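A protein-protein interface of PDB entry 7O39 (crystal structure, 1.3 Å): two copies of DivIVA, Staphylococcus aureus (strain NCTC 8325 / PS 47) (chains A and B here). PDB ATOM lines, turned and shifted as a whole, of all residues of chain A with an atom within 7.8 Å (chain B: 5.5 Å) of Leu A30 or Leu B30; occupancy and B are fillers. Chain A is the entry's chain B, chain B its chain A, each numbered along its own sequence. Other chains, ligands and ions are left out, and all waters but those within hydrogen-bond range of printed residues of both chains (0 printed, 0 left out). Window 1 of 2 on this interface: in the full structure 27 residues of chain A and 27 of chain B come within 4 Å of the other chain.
Among the printed residues, pairs that only touch across the chains: Glu A25 with Phe B14, Phe A14 with Glu B25, Lys A12 with Phe B29, Leu A33 with Leu B30, Leu A30 with Leu B33, Leu A30 with Leu B30, Ile A9 with Leu B33, Val A26 with Phe B14, Phe A14 with Val B26, Leu A21 with Val B26, Leu A33 with Ile B9, Phe A29 with Phe B14, Phe A14 with Phe B29, Leu A30 with Phe B29, Phe A29 with Leu B30, Leu A21 with Phe B14, Val A26 with Val B26 and Leu A33 with Leu B33.
Glu A8 touches none of the printed residues of chain B. Printed residues of chain B within 4 Å of Ile A9: Leu B33 (3.7 Å). Of the printed residues of chain B, Leu A21 touches Phe B14 (3.9 Å) and Val B26 (3.8 Å). Leu A30 touches just these residues of chain B: Phe B29 (3.9 Å), Leu B30 (3.7 Å) and Leu B33 (3.7 Å). Glu A36 touches none of the printed residues of chain B. Of the printed residues of chain A, Ile B9 touches Leu A33. Of the printed residues of chain A, Phe B14 touches Leu A21 (3.9 Å), Glu A25 (3.4 Å), Val A26 (3.8 Å) and Phe A29 (3.9 Å). Leu B30 touches just these residues of chain A: Phe A29 (3.9 Å), Leu A30 (3.7 Å) and Leu A33 (3.7 Å). Of the printed residues of chain A, Leu B33 touches Ile A9, Leu A30 and Leu A33. The nearest printed residue of chain B that does not touch Leu A30 is Val B26 (6.1 Å). The nearest residue of chain A that does not touch Leu B30 is Val A26 (6.0 Å). The nearest printed residue of chain A that does not touch Leu B33 is Ile A37 (4.03 Å).
Printed residues of chain B that touch a printed residue of chain A: Ile B9, Phe B14, Glu B25, Val B26, Phe B29, Leu B30 and Leu B33. Among the printed residues, no Asp or Glu carboxylate lies within 4 Å of a Lys or Arg side-chain nitrogen of the other chain.
Phe A14 touches Phe B29, and with the chains exchanged Phe A29 touches Phe B14. Val A26 touches its own counterpart, Val B26. Phe A29 touches Leu B30, and with the chains exchanged Leu A30 touches Phe B29. Leu A33 touches its own counterpart, Leu B33. Positions printed for both chains: 9, 14, 25, 26, 27, 28, 29, 30, 31, 32, 33, 34 and 35. Of the 18 pairs that touch across the chains among the printed residues, 15 have their exchanged pair printed and touching as well.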
ATOM      1  N   PRO A   6      38.524 -10.146   5.252  1.00  0.00           N
ATOM      2  CA  PRO A   6      37.780 -11.282   4.690  1.00  0.00           C
ATOM      3  C   PRO A   6      37.969 -12.572   5.469  1.00  0.00           C
ATOM      4  O   PRO A   6      36.999 -13.313   5.665  1.00  0.00           O
ATOM      5  CB  PRO A   6      38.315 -11.366   3.253  1.00  0.00           C
ATOM      6  CG  PRO A   6      38.702  -9.959   2.941  1.00  0.00           C
ATOM      7  CD  PRO A   6      39.299  -9.440   4.219  1.00  0.00           C
ATOM      8  N   GLU A   8      38.583 -12.984   8.681  1.00  0.00           N
ATOM      9  CA  GLU A   8      37.774 -12.904   9.896  1.00  0.00           C
ATOM     10  C   GLU A   8      36.295 -13.091   9.578  1.00  0.00           C
ATOM     11  O   GLU A   8      35.604 -13.885  10.226  1.00  0.00           O
ATOM     12  CB  GLU A   8      37.978 -11.557  10.593  1.00  0.00           C
ATOM     13  CG  GLU A   8      39.395 -11.250  11.035  1.00  0.00           C
ATOM     14  CD  GLU A   8      39.519  -9.854  11.620  1.00  0.00           C
ATOM     15  OE1 GLU A   8      39.754  -8.898  10.847  1.00  0.00           O
ATOM     16  OE2 GLU A   8      39.370  -9.709  12.851  1.00  0.00           O
ATOM     17  N   ILE A   9      35.787 -12.354   8.587  1.00  0.00           N
ATOM     18  CA  ILE A   9      34.364 -12.433   8.266  1.00  0.00           C
ATOM     19  C   ILE A   9      34.009 -13.833   7.785  1.00  0.00           C
ATOM     20  O   ILE A   9      32.966 -14.390   8.153  1.00  0.00           O
ATOM     21  CB  ILE A   9      33.987 -11.359   7.225  1.00  0.00           C
ATOM     22  CG1 ILE A   9      34.221  -9.956   7.792  1.00  0.00           C
ATOM     23  CG2 ILE A   9      32.530 -11.521   6.784  1.00  0.00           C
ATOM     24  CD1 ILE A   9      34.140  -8.846   6.755  1.00  0.00           C
ATOM     25  N   LYS A  10      34.869 -14.424   6.955  1.00  0.00           N
ATOM     26  CA  LYS A  10      34.580 -15.735   6.392  1.00  0.00           C
ATOM     27  C   LYS A  10      34.732 -16.852   7.414  1.00  0.00           C
ATOM     28  O   LYS A  10      34.181 -17.939   7.209  1.00  0.00           O
ATOM     29  CB  LYS A  10      35.498 -15.990   5.199  1.00  0.00           C
ATOM     30  CG  LYS A  10      35.162 -15.144   3.983  1.00  0.00           C
ATOM     31  N   ASN A  11      35.459 -16.612   8.503  1.00  0.00           N
ATOM     32  CA  ASN A  11      35.613 -17.582   9.578  1.00  0.00           C
ATOM     33  C   ASN A  11      34.856 -17.150  10.826  1.00  0.00           C
ATOM     34  O   ASN A  11      35.182 -17.583  11.935  1.00  0.00           O
ATOM     35  CB  ASN A  11      37.093 -17.807   9.882  1.00  0.00           C
ATOM     36  CG  ASN A  11      37.775 -18.655   8.827  1.00  0.00           C
ATOM     37  OD1 ASN A  11      37.111 -19.283   8.000  1.00  0.00           O
ATOM     38  ND2 ASN A  11      39.101 -18.670   8.840  1.00  0.00           N
ATOM     39  N   LYS A  12      33.853 -16.298  10.658  1.00  0.00           N
ATOM     40  CA  LYS A  12      33.100 -15.765  11.779  1.00  0.00           C
ATOM     41  C   LYS A  12      32.175 -16.843  12.318  1.00  0.00           C
ATOM     42  O   LYS A  12      31.247 -17.279  11.627  1.00  0.00           O
ATOM     43  CB  LYS A  12      32.281 -14.572  11.299  1.00  0.00           C
ATOM     44  CG  LYS A  12      31.693 -13.686  12.385  1.00  0.00           C
ATOM     45  CD  LYS A  12      32.581 -13.583  13.602  1.00  0.00           C
ATOM     46  CE  LYS A  12      32.246 -12.377  14.450  1.00  0.00           C
ATOM     47  NZ  LYS A  12      31.276 -12.698  15.524  1.00  0.00           N
ATOM     48  N   GLU A  13      32.421 -17.271  13.548  1.00  0.00           N
ATOM     49  CA  GLU A  13      31.526 -18.200  14.217  1.00  0.00           C
ATOM     50  C   GLU A  13      30.585 -17.422  15.125  1.00  0.00           C
ATOM     51  O   GLU A  13      30.895 -16.321  15.594  1.00  0.00           O
ATOM     52  CB  GLU A  13      32.291 -19.262  15.016  1.00  0.00           C
ATOM     53  CG  GLU A  13      33.316 -20.054  14.193  1.00  0.00           C
ATOM     54  CD  GLU A  13      32.759 -21.326  13.538  1.00  0.00           C
ATOM     55  OE1 GLU A  13      31.536 -21.594  13.598  1.00  0.00           O
ATOM     56  OE2 GLU A  13      33.571 -22.062  12.942  1.00  0.00           O
ATOM     57  N   PHE A  14      29.408 -17.990  15.318  1.00  0.00           N
ATOM     58  CA  PHE A  14      28.404 -17.467  16.224  1.00  0.00           C
ATOM     59  C   PHE A  14      27.953 -18.608  17.115  1.00  0.00           C
ATOM     60  O   PHE A  14      28.053 -19.779  16.740  1.00  0.00           O
ATOM     61  CB  PHE A  14      27.204 -16.933  15.449  1.00  0.00           C
ATOM     62  CG  PHE A  14      27.543 -15.810  14.518  1.00  0.00           C
ATOM     63  CD1 PHE A  14      27.547 -14.511  14.973  1.00  0.00           C
ATOM     64  CD2 PHE A  14      27.853 -16.057  13.194  1.00  0.00           C
ATOM     65  CE1 PHE A  14      27.868 -13.468  14.119  1.00  0.00           C
ATOM     66  CE2 PHE A  14      28.165 -15.028  12.342  1.00  0.00           C
ATOM     67  CZ  PHE A  14      28.166 -13.734  12.801  1.00  0.00           C
ATOM     68  N   LEU A  21      19.181 -18.615  13.401  1.00  0.00           N
ATOM     69  CA  LEU A  21      19.190 -18.277  11.990  1.00  0.00           C
ATOM     70  C   LEU A  21      19.899 -19.352  11.174  1.00  0.00           C
ATOM     71  O   LEU A  21      20.903 -19.932  11.610  1.00  0.00           O
ATOM     72  CB  LEU A  21      19.925 -16.949  11.788  1.00  0.00           C
ATOM     73  CG  LEU A  21      19.451 -15.754  12.623  1.00  0.00           C
ATOM     74  CD1 LEU A  21      20.223 -14.501  12.210  1.00  0.00           C
ATOM     75  CD2 LEU A  21      17.947 -15.527  12.504  1.00  0.00           C
ATOM     76  N   PRO A  23      22.352 -21.155   9.194  1.00  0.00           N
ATOM     77  CA  PRO A  23      23.778 -20.763   9.150  1.00  0.00           C
ATOM     78  C   PRO A  23      24.311 -20.477   7.761  1.00  0.00           C
ATOM     79  O   PRO A  23      25.153 -19.576   7.598  1.00  0.00           O
ATOM     80  CB  PRO A  23      24.494 -21.946   9.824  1.00  0.00           C
ATOM     81  CG  PRO A  23      23.462 -22.493  10.754  1.00  0.00           C
ATOM     82  CD  PRO A  23      22.160 -22.372  10.004  1.00  0.00           C
ATOM     83  N   THR A  24      23.848 -21.213   6.750  1.00  0.00           N
ATOM     84  CA  THR A  24      24.372 -21.022   5.402  1.00  0.00           C
ATOM     85  C   THR A  24      23.854 -19.725   4.785  1.00  0.00           C
ATOM     86  O   THR A  24      24.607 -19.014   4.106  1.00  0.00           O
ATOM     87  CB  THR A  24      24.051 -22.246   4.544  1.00  0.00           C
ATOM     88  OG1 THR A  24      24.649 -23.397   5.152  1.00  0.00           O
ATOM     89  CG2 THR A  24      24.602 -22.086   3.130  1.00  0.00           C
ATOM     90  N   GLU A  25      22.580 -19.388   5.015  1.00  0.00           N
ATOM     91  CA  GLU A  25      22.065 -18.098   4.547  1.00  0.00           C
ATOM     92  C   GLU A  25      22.875 -16.945   5.128  1.00  0.00           C
ATOM     93  O   GLU A  25      23.226 -15.991   4.416  1.00  0.00           O
ATOM     94  CB  GLU A  25      20.593 -17.912   4.925  1.00  0.00           C
ATOM     95  CG  GLU A  25      19.602 -18.850   4.260  1.00  0.00           C
ATOM     96  CD  GLU A  25      18.175 -18.687   4.791  1.00  0.00           C
ATOM     97  OE1 GLU A  25      17.892 -17.665   5.454  1.00  0.00           O
ATOM     98  OE2 GLU A  25      17.344 -19.590   4.544  1.00  0.00           O
ATOM     99  N   VAL A  26      23.193 -17.012   6.421  1.00  0.00           N
ATOM    100  CA  VAL A  26      23.992 -15.956   7.033  1.00  0.00           C
ATOM    101  C   VAL A  26      25.381 -15.921   6.409  1.00  0.00           C
ATOM    102  O   VAL A  26      25.884 -14.857   6.034  1.00  0.00           O
ATOM    103  CB  VAL A  26      24.040 -16.129   8.560  1.00  0.00           C
ATOM    104  CG1 VAL A  26      25.008 -15.136   9.177  1.00  0.00           C
ATOM    105  CG2 VAL A  26      22.652 -15.942   9.149  1.00  0.00           C
ATOM    106  N   ALA A  27      26.025 -17.078   6.279  1.00  0.00           N
ATOM    107  CA  ALA A  27      27.363 -17.109   5.696  1.00  0.00           C
ATOM    108  C   ALA A  27      27.368 -16.506   4.298  1.00  0.00           C
ATOM    109  O   ALA A  27      28.301 -15.776   3.934  1.00  0.00           O
ATOM    110  CB  ALA A  27      27.869 -18.544   5.649  1.00  0.00           C
ATOM    111  N   ASN A  28      26.358 -16.814   3.478  1.00  0.00           N
ATOM    112  CA  ASN A  28      26.342 -16.296   2.113  1.00  0.00           C
ATOM    113  C   ASN A  28      26.210 -14.781   2.106  1.00  0.00           C
ATOM    114  O   ASN A  28      26.822 -14.095   1.273  1.00  0.00           O
ATOM    115  CB  ASN A  28      25.198 -16.928   1.328  1.00  0.00           C
ATOM    116  CG  ASN A  28      25.418 -18.399   1.055  1.00  0.00           C
ATOM    117  OD1 ASN A  28      26.539 -18.892   1.103  1.00  0.00           O
ATOM    118  ND2 ASN A  28      24.337 -19.109   0.757  1.00  0.00           N
ATOM    119  N   PHE A  29      25.411 -14.234   3.017  1.00  0.00           N
ATOM    120  CA  PHE A  29      25.291 -12.782   3.107  1.00  0.00           C
ATOM    121  C   PHE A  29      26.585 -12.150   3.609  1.00  0.00           C
ATOM    122  O   PHE A  29      27.020 -11.108   3.096  1.00  0.00           O
ATOM    123  CB  PHE A  29      24.115 -12.417   4.004  1.00  0.00           C
ATOM    124  CG  PHE A  29      23.707 -10.975   3.931  1.00  0.00           C
ATOM    125  CD1 PHE A  29      23.388 -10.384   2.721  1.00  0.00           C
ATOM    126  CD2 PHE A  29      23.620 -10.209   5.078  1.00  0.00           C
ATOM    127  CE1 PHE A  29      22.993  -9.061   2.666  1.00  0.00           C
ATOM    128  CE2 PHE A  29      23.205  -8.895   5.019  1.00  0.00           C
ATOM    129  CZ  PHE A  29      22.905  -8.324   3.822  1.00  0.00           C
ATOM    130  N   LEU A  30      27.228 -12.769   4.591  1.00  0.00           N
ATOM    131  CA  LEU A  30      28.509 -12.253   5.066  1.00  0.00           C
ATOM    132  C   LEU A  30      29.553 -12.251   3.958  1.00  0.00           C
ATOM    133  O   LEU A  30      30.379 -11.333   3.887  1.00  0.00           O
ATOM    134  CB  LEU A  30      29.005 -13.069   6.257  1.00  0.00           C
ATOM    135  CG  LEU A  30      28.176 -12.927   7.529  1.00  0.00           C
ATOM    136  CD1 LEU A  30      28.761 -13.841   8.588  1.00  0.00           C
ATOM    137  CD2 LEU A  30      28.136 -11.494   8.017  1.00  0.00           C
ATOM    138  N   GLU A  31      29.532 -13.258   3.076  1.00  0.00           N
ATOM    139  CA  GLU A  31      30.454 -13.269   1.943  1.00  0.00           C
ATOM    140  C   GLU A  31      30.212 -12.070   1.040  1.00  0.00           C
ATOM    141  O   GLU A  31      31.164 -11.429   0.578  1.00  0.00           O
ATOM    142  CB  GLU A  31      30.317 -14.574   1.154  1.00  0.00           C
ATOM    143  CG  GLU A  31      31.225 -14.639  -0.085  1.00  0.00           C
ATOM    144  CD  GLU A  31      31.003 -15.877  -0.946  1.00  0.00           C
ATOM    145  OE1 GLU A  31      29.929 -16.508  -0.848  1.00  0.00           O
ATOM    146  OE2 GLU A  31      31.912 -16.212  -1.742  1.00  0.00           O
ATOM    147  N   GLN A  32      28.946 -11.732   0.784  1.00  0.00           N
ATOM    148  CA  GLN A  32      28.637 -10.568  -0.039  1.00  0.00           C
ATOM    149  C   GLN A  32      29.144  -9.287   0.606  1.00  0.00           C
ATOM    150  O   GLN A  32      29.689  -8.417  -0.080  1.00  0.00           O
ATOM    151  CB  GLN A  32      27.138 -10.485  -0.318  1.00  0.00           C
ATOM    152  CG  GLN A  32      26.634 -11.614  -1.208  1.00  0.00           C
ATOM    153  CD  GLN A  32      25.149 -11.549  -1.451  1.00  0.00           C
ATOM    154  OE1 GLN A  32      24.370 -11.297  -0.534  1.00  0.00           O
ATOM    155  NE2 GLN A  32      24.737 -11.846  -2.673  1.00  0.00           N
ATOM    156  N   LEU A  33      28.985  -9.159   1.923  1.00  0.00           N
ATOM    157  CA  LEU A  33      29.426  -7.950   2.605  1.00  0.00           C
ATOM    158  C   LEU A  33      30.943  -7.856   2.629  1.00  0.00           C
ATOM    159  O   LEU A  33      31.504  -6.772   2.439  1.00  0.00           O
ATOM    160  CB  LEU A  33      28.847  -7.906   4.017  1.00  0.00           C
ATOM    161  CG  LEU A  33      27.320  -7.777   4.076  1.00  0.00           C
ATOM    162  CD1 LEU A  33      26.846  -7.714   5.524  1.00  0.00           C
ATOM    163  CD2 LEU A  33      26.795  -6.569   3.310  1.00  0.00           C
ATOM    164  N   SER A  34      31.625  -8.973   2.869  1.00  0.00           N
ATOM    165  CA  SER A  34      33.080  -8.969   2.838  1.00  0.00           C
ATOM    166  C   SER A  34      33.583  -8.554   1.459  1.00  0.00           C
ATOM    167  O   SER A  34      34.539  -7.778   1.340  1.00  0.00           O
ATOM    168  CB  SER A  34      33.620 -10.341   3.230  1.00  0.00           C
ATOM    169  OG  SER A  34      35.030 -10.350   3.104  1.00  0.00           O
ATOM    170  N   THR A  35      32.959  -9.076   0.401  1.00  0.00           N
ATOM    171  CA  THR A  35      33.353  -8.715  -0.957  1.00  0.00           C
ATOM    172  C   THR A  35      33.169  -7.222  -1.188  1.00  0.00           C
ATOM    173  O   THR A  35      34.032  -6.559  -1.784  1.00  0.00           O
ATOM    174  CB  THR A  35      32.551  -9.547  -1.960  1.00  0.00           C
ATOM    175  OG1 THR A  35      32.891 -10.930  -1.804  1.00  0.00           O
ATOM    176  CG2 THR A  35      32.842  -9.114  -3.385  1.00  0.00           C
ATOM    177  N   GLU A  36      32.057  -6.667  -0.707  1.00  0.00           N
ATOM    178  CA  GLU A  36      31.820  -5.238  -0.862  1.00  0.00           C
ATOM    179  C   GLU A  36      32.899  -4.428  -0.157  1.00  0.00           C
ATOM    180  O   GLU A  36      33.431  -3.459  -0.720  1.00  0.00           O
ATOM    181  CB  GLU A  36      30.430  -4.877  -0.340  1.00  0.00           C
ATOM    182  CG  GLU A  36      30.087  -3.383  -0.415  1.00  0.00           C
ATOM    183  CD  GLU A  36      29.967  -2.833  -1.825  1.00  0.00           C
ATOM    184  OE1 GLU A  36      30.114  -3.601  -2.800  1.00  0.00           O
ATOM    185  OE2 GLU A  36      29.730  -1.611  -1.962  1.00  0.00           O
ATOM    186  N   ILE A  37      33.248  -4.817   1.074  1.00  0.00           N
ATOM    187  CA  ILE A  37      34.305  -4.120   1.805  1.00  0.00           C
ATOM    188  C   ILE A  37      35.630  -4.188   1.039  1.00  0.00           C
ATOM    189  O   ILE A  37      36.342  -3.182   0.891  1.00  0.00           O
ATOM    190  CB  ILE A  37      34.414  -4.710   3.225  1.00  0.00           C
ATOM    191  CG1 ILE A  37      33.194  -4.289   4.055  1.00  0.00           C
ATOM    192  CG2 ILE A  37      35.721  -4.313   3.893  1.00  0.00           C
ATOM    193  CD1 ILE A  37      33.009  -5.068   5.360  1.00  0.00           C
ATOM    194  N   ILE B   9      20.918  -3.928   4.964  1.00  0.00           N
ATOM    195  CA  ILE B   9      21.668  -4.892   5.760  1.00  0.00           C
ATOM    196  C   ILE B   9      20.896  -5.252   7.015  1.00  0.00           C
ATOM    197  O   ILE B   9      20.744  -6.429   7.357  1.00  0.00           O
ATOM    198  CB  ILE B   9      23.061  -4.332   6.097  1.00  0.00           C
ATOM    199  CG1 ILE B   9      23.894  -4.233   4.821  1.00  0.00           C
ATOM    200  CG2 ILE B   9      23.746  -5.189   7.170  1.00  0.00           C
ATOM    201  CD1 ILE B   9      25.203  -3.505   4.994  1.00  0.00           C
ATOM    202  N   PHE B  14      16.368 -13.801   7.621  1.00  0.00           N
ATOM    203  CA  PHE B  14      16.915 -15.141   7.522  1.00  0.00           C
ATOM    204  C   PHE B  14      15.896 -16.136   8.051  1.00  0.00           C
ATOM    205  O   PHE B  14      15.162 -15.859   9.008  1.00  0.00           O
ATOM    206  CB  PHE B  14      18.203 -15.264   8.333  1.00  0.00           C
ATOM    207  CG  PHE B  14      19.282 -14.316   7.886  1.00  0.00           C
ATOM    208  CD1 PHE B  14      20.037 -14.593   6.769  1.00  0.00           C
ATOM    209  CD2 PHE B  14      19.524 -13.146   8.577  1.00  0.00           C
ATOM    210  CE1 PHE B  14      21.020 -13.730   6.351  1.00  0.00           C
ATOM    211  CE2 PHE B  14      20.503 -12.283   8.166  1.00  0.00           C
ATOM    212  CZ  PHE B  14      21.248 -12.576   7.049  1.00  0.00           C
ATOM    213  N   GLU B  25      23.604 -11.950  18.097  1.00  0.00           N
ATOM    214  CA  GLU B  25      25.014 -11.900  17.725  1.00  0.00           C
ATOM    215  C   GLU B  25      25.166 -11.571  16.252  1.00  0.00           C
ATOM    216  O   GLU B  25      26.022 -10.760  15.867  1.00  0.00           O
ATOM    217  CB  GLU B  25      25.695 -13.236  18.013  1.00  0.00           C
ATOM    218  CG  GLU B  25      25.833 -13.590  19.482  1.00  0.00           C
ATOM    219  CD  GLU B  25      26.515 -14.933  19.708  1.00  0.00           C
ATOM    220  OE1 GLU B  25      27.131 -15.481  18.762  1.00  0.00           O
ATOM    221  OE2 GLU B  25      26.420 -15.443  20.846  1.00  0.00           O
ATOM    222  N   VAL B  26      24.346 -12.197  15.410  1.00  0.00           N
ATOM    223  CA  VAL B  26      24.404 -11.920  13.978  1.00  0.00           C
ATOM    224  C   VAL B  26      24.015 -10.470  13.698  1.00  0.00           C
ATOM    225  O   VAL B  26      24.708  -9.758  12.962  1.00  0.00           O
ATOM    226  CB  VAL B  26      23.533 -12.920  13.194  1.00  0.00           C
ATOM    227  CG1 VAL B  26      23.455 -12.525  11.716  1.00  0.00           C
ATOM    228  CG2 VAL B  26      24.084 -14.336  13.331  1.00  0.00           C
ATOM    229  N   ALA B  27      22.893 -10.010  14.273  1.00  0.00           N
ATOM    230  CA  ALA B  27      22.452  -8.632  14.050  1.00  0.00           C
ATOM    231  C   ALA B  27      23.538  -7.639  14.444  1.00  0.00           C
ATOM    232  O   ALA B  27      23.789  -6.656  13.729  1.00  0.00           O
ATOM    233  CB  ALA B  27      21.159  -8.345  14.813  1.00  0.00           C
ATOM    234  N   ASN B  28      24.194  -7.871  15.584  1.00  0.00           N
ATOM    235  CA  ASN B  28      25.217  -6.937  16.041  1.00  0.00           C
ATOM    236  C   ASN B  28      26.405  -6.906  15.089  1.00  0.00           C
ATOM    237  O   ASN B  28      26.964  -5.836  14.813  1.00  0.00           O
ATOM    238  CB  ASN B  28      25.660  -7.310  17.455  1.00  0.00           C
ATOM    239  CG  ASN B  28      24.599  -7.000  18.508  1.00  0.00           C
ATOM    240  OD1 ASN B  28      23.681  -6.212  18.273  1.00  0.00           O
ATOM    241  ND2 ASN B  28      24.728  -7.618  19.674  1.00  0.00           N
ATOM    242  N   PHE B  29      26.787  -8.067  14.553  1.00  0.00           N
ATOM    243  CA  PHE B  29      27.909  -8.122  13.625  1.00  0.00           C
ATOM    244  C   PHE B  29      27.557  -7.456  12.305  1.00  0.00           C
ATOM    245  O   PHE B  29      28.380  -6.733  11.728  1.00  0.00           O
ATOM    246  CB  PHE B  29      28.325  -9.574  13.401  1.00  0.00           C
ATOM    247  CG  PHE B  29      29.631  -9.728  12.670  1.00  0.00           C
ATOM    248  CD1 PHE B  29      30.808  -9.227  13.202  1.00  0.00           C
ATOM    249  CD2 PHE B  29      29.683 -10.388  11.454  1.00  0.00           C
ATOM    250  CE1 PHE B  29      32.007  -9.369  12.525  1.00  0.00           C
ATOM    251  CE2 PHE B  29      30.881 -10.542  10.786  1.00  0.00           C
ATOM    252  CZ  PHE B  29      32.037 -10.031  11.319  1.00  0.00           C
ATOM    253  N   LEU B  30      26.331  -7.665  11.819  1.00  0.00           N
ATOM    254  CA  LEU B  30      25.900  -6.996  10.598  1.00  0.00           C
ATOM    255  C   LEU B  30      25.909  -5.482  10.769  1.00  0.00           C
ATOM    256  O   LEU B  30      26.276  -4.752   9.840  1.00  0.00           O
ATOM    257  CB  LEU B  30      24.510  -7.491  10.203  1.00  0.00           C
ATOM    258  CG  LEU B  30      24.436  -8.944   9.736  1.00  0.00           C
ATOM    259  CD1 LEU B  30      22.985  -9.288   9.474  1.00  0.00           C
ATOM    260  CD2 LEU B  30      25.286  -9.196   8.497  1.00  0.00           C
ATOM    261  N   GLU B  31      25.533  -4.992  11.952  1.00  0.00           N
ATOM    262  CA  GLU B  31      25.600  -3.554  12.207  1.00  0.00           C
ATOM    263  C   GLU B  31      27.038  -3.045  12.115  1.00  0.00           C
ATOM    264  O   GLU B  31      27.293  -1.978  11.543  1.00  0.00           O
ATOM    265  CB  GLU B  31      24.987  -3.237  13.575  1.00  0.00           C
ATOM    266  CG  GLU B  31      24.952  -1.760  13.950  1.00  0.00           C
ATOM    267  CD  GLU B  31      24.283  -1.512  15.295  1.00  0.00           C
ATOM    268  OE1 GLU B  31      24.311  -2.413  16.158  1.00  0.00           O
ATOM    269  OE2 GLU B  31      23.734  -0.406  15.488  1.00  0.00           O
ATOM    270  N   GLN B  32      27.993  -3.811  12.649  1.00  0.00           N
ATOM    271  CA  GLN B  32      29.400  -3.429  12.549  1.00  0.00           C
ATOM    272  C   GLN B  32      29.868  -3.409  11.100  1.00  0.00           C
ATOM    273  O   GLN B  32      30.615  -2.505  10.692  1.00  0.00           O
ATOM    274  CB  GLN B  32      30.262  -4.375  13.377  1.00  0.00           C
ATOM    275  CG  GLN B  32      30.057  -4.254  14.884  1.00  0.00           C
ATOM    276  CD  GLN B  32      30.990  -5.160  15.656  1.00  0.00           C
ATOM    277  OE1 GLN B  32      30.940  -6.385  15.523  1.00  0.00           O
ATOM    278  NE2 GLN B  32      31.855  -4.561  16.464  1.00  0.00           N
ATOM    279  N   LEU B  33      29.459  -4.401  10.306  1.00  0.00           N
ATOM    280  CA  LEU B  33      29.868  -4.421   8.906  1.00  0.00           C
ATOM    281  C   LEU B  33      29.256  -3.257   8.137  1.00  0.00           C
ATOM    282  O   LEU B  33      29.923  -2.655   7.282  1.00  0.00           O
ATOM    283  CB  LEU B  33      29.505  -5.752   8.250  1.00  0.00           C
ATOM    284  CG  LEU B  33      30.250  -6.965   8.816  1.00  0.00           C
ATOM    285  CD1 LEU B  33      29.848  -8.229   8.072  1.00  0.00           C
ATOM    286  CD2 LEU B  33      31.763  -6.786   8.787  1.00  0.00           C
ATOM    287  N   SER B  34      28.003  -2.910   8.432  1.00  0.00           N
ATOM    288  CA  SER B  34      27.391  -1.752   7.786  1.00  0.00           C
ATOM    289  C   SER B  34      28.163  -0.475   8.100  1.00  0.00           C
ATOM    290  O   SER B  34      28.409   0.350   7.213  1.00  0.00           O
ATOM    291  CB  SER B  34      25.935  -1.613   8.209  1.00  0.00           C
ATOM    292  OG  SER B  34      25.379  -0.470   7.590  1.00  0.00           O
ATOM    293  N   THR B  35      28.546  -0.294   9.360  1.00  0.00           N
ATOM    294  CA  THR B  35      29.340   0.871   9.728  1.00  0.00           C
ATOM    295  C   THR B  35      30.643   0.917   8.937  1.00  0.00           C
ATOM    296  O   THR B  35      31.042   1.979   8.449  1.00  0.00           O
ATOM    297  CB  THR B  35      29.587   0.855  11.238  1.00  0.00           C
ATOM    298  OG1 THR B  35      28.334   1.016  11.905  1.00  0.00           O
ATOM    299  CG2 THR B  35      30.521   1.978  11.674  1.00  0.00           C
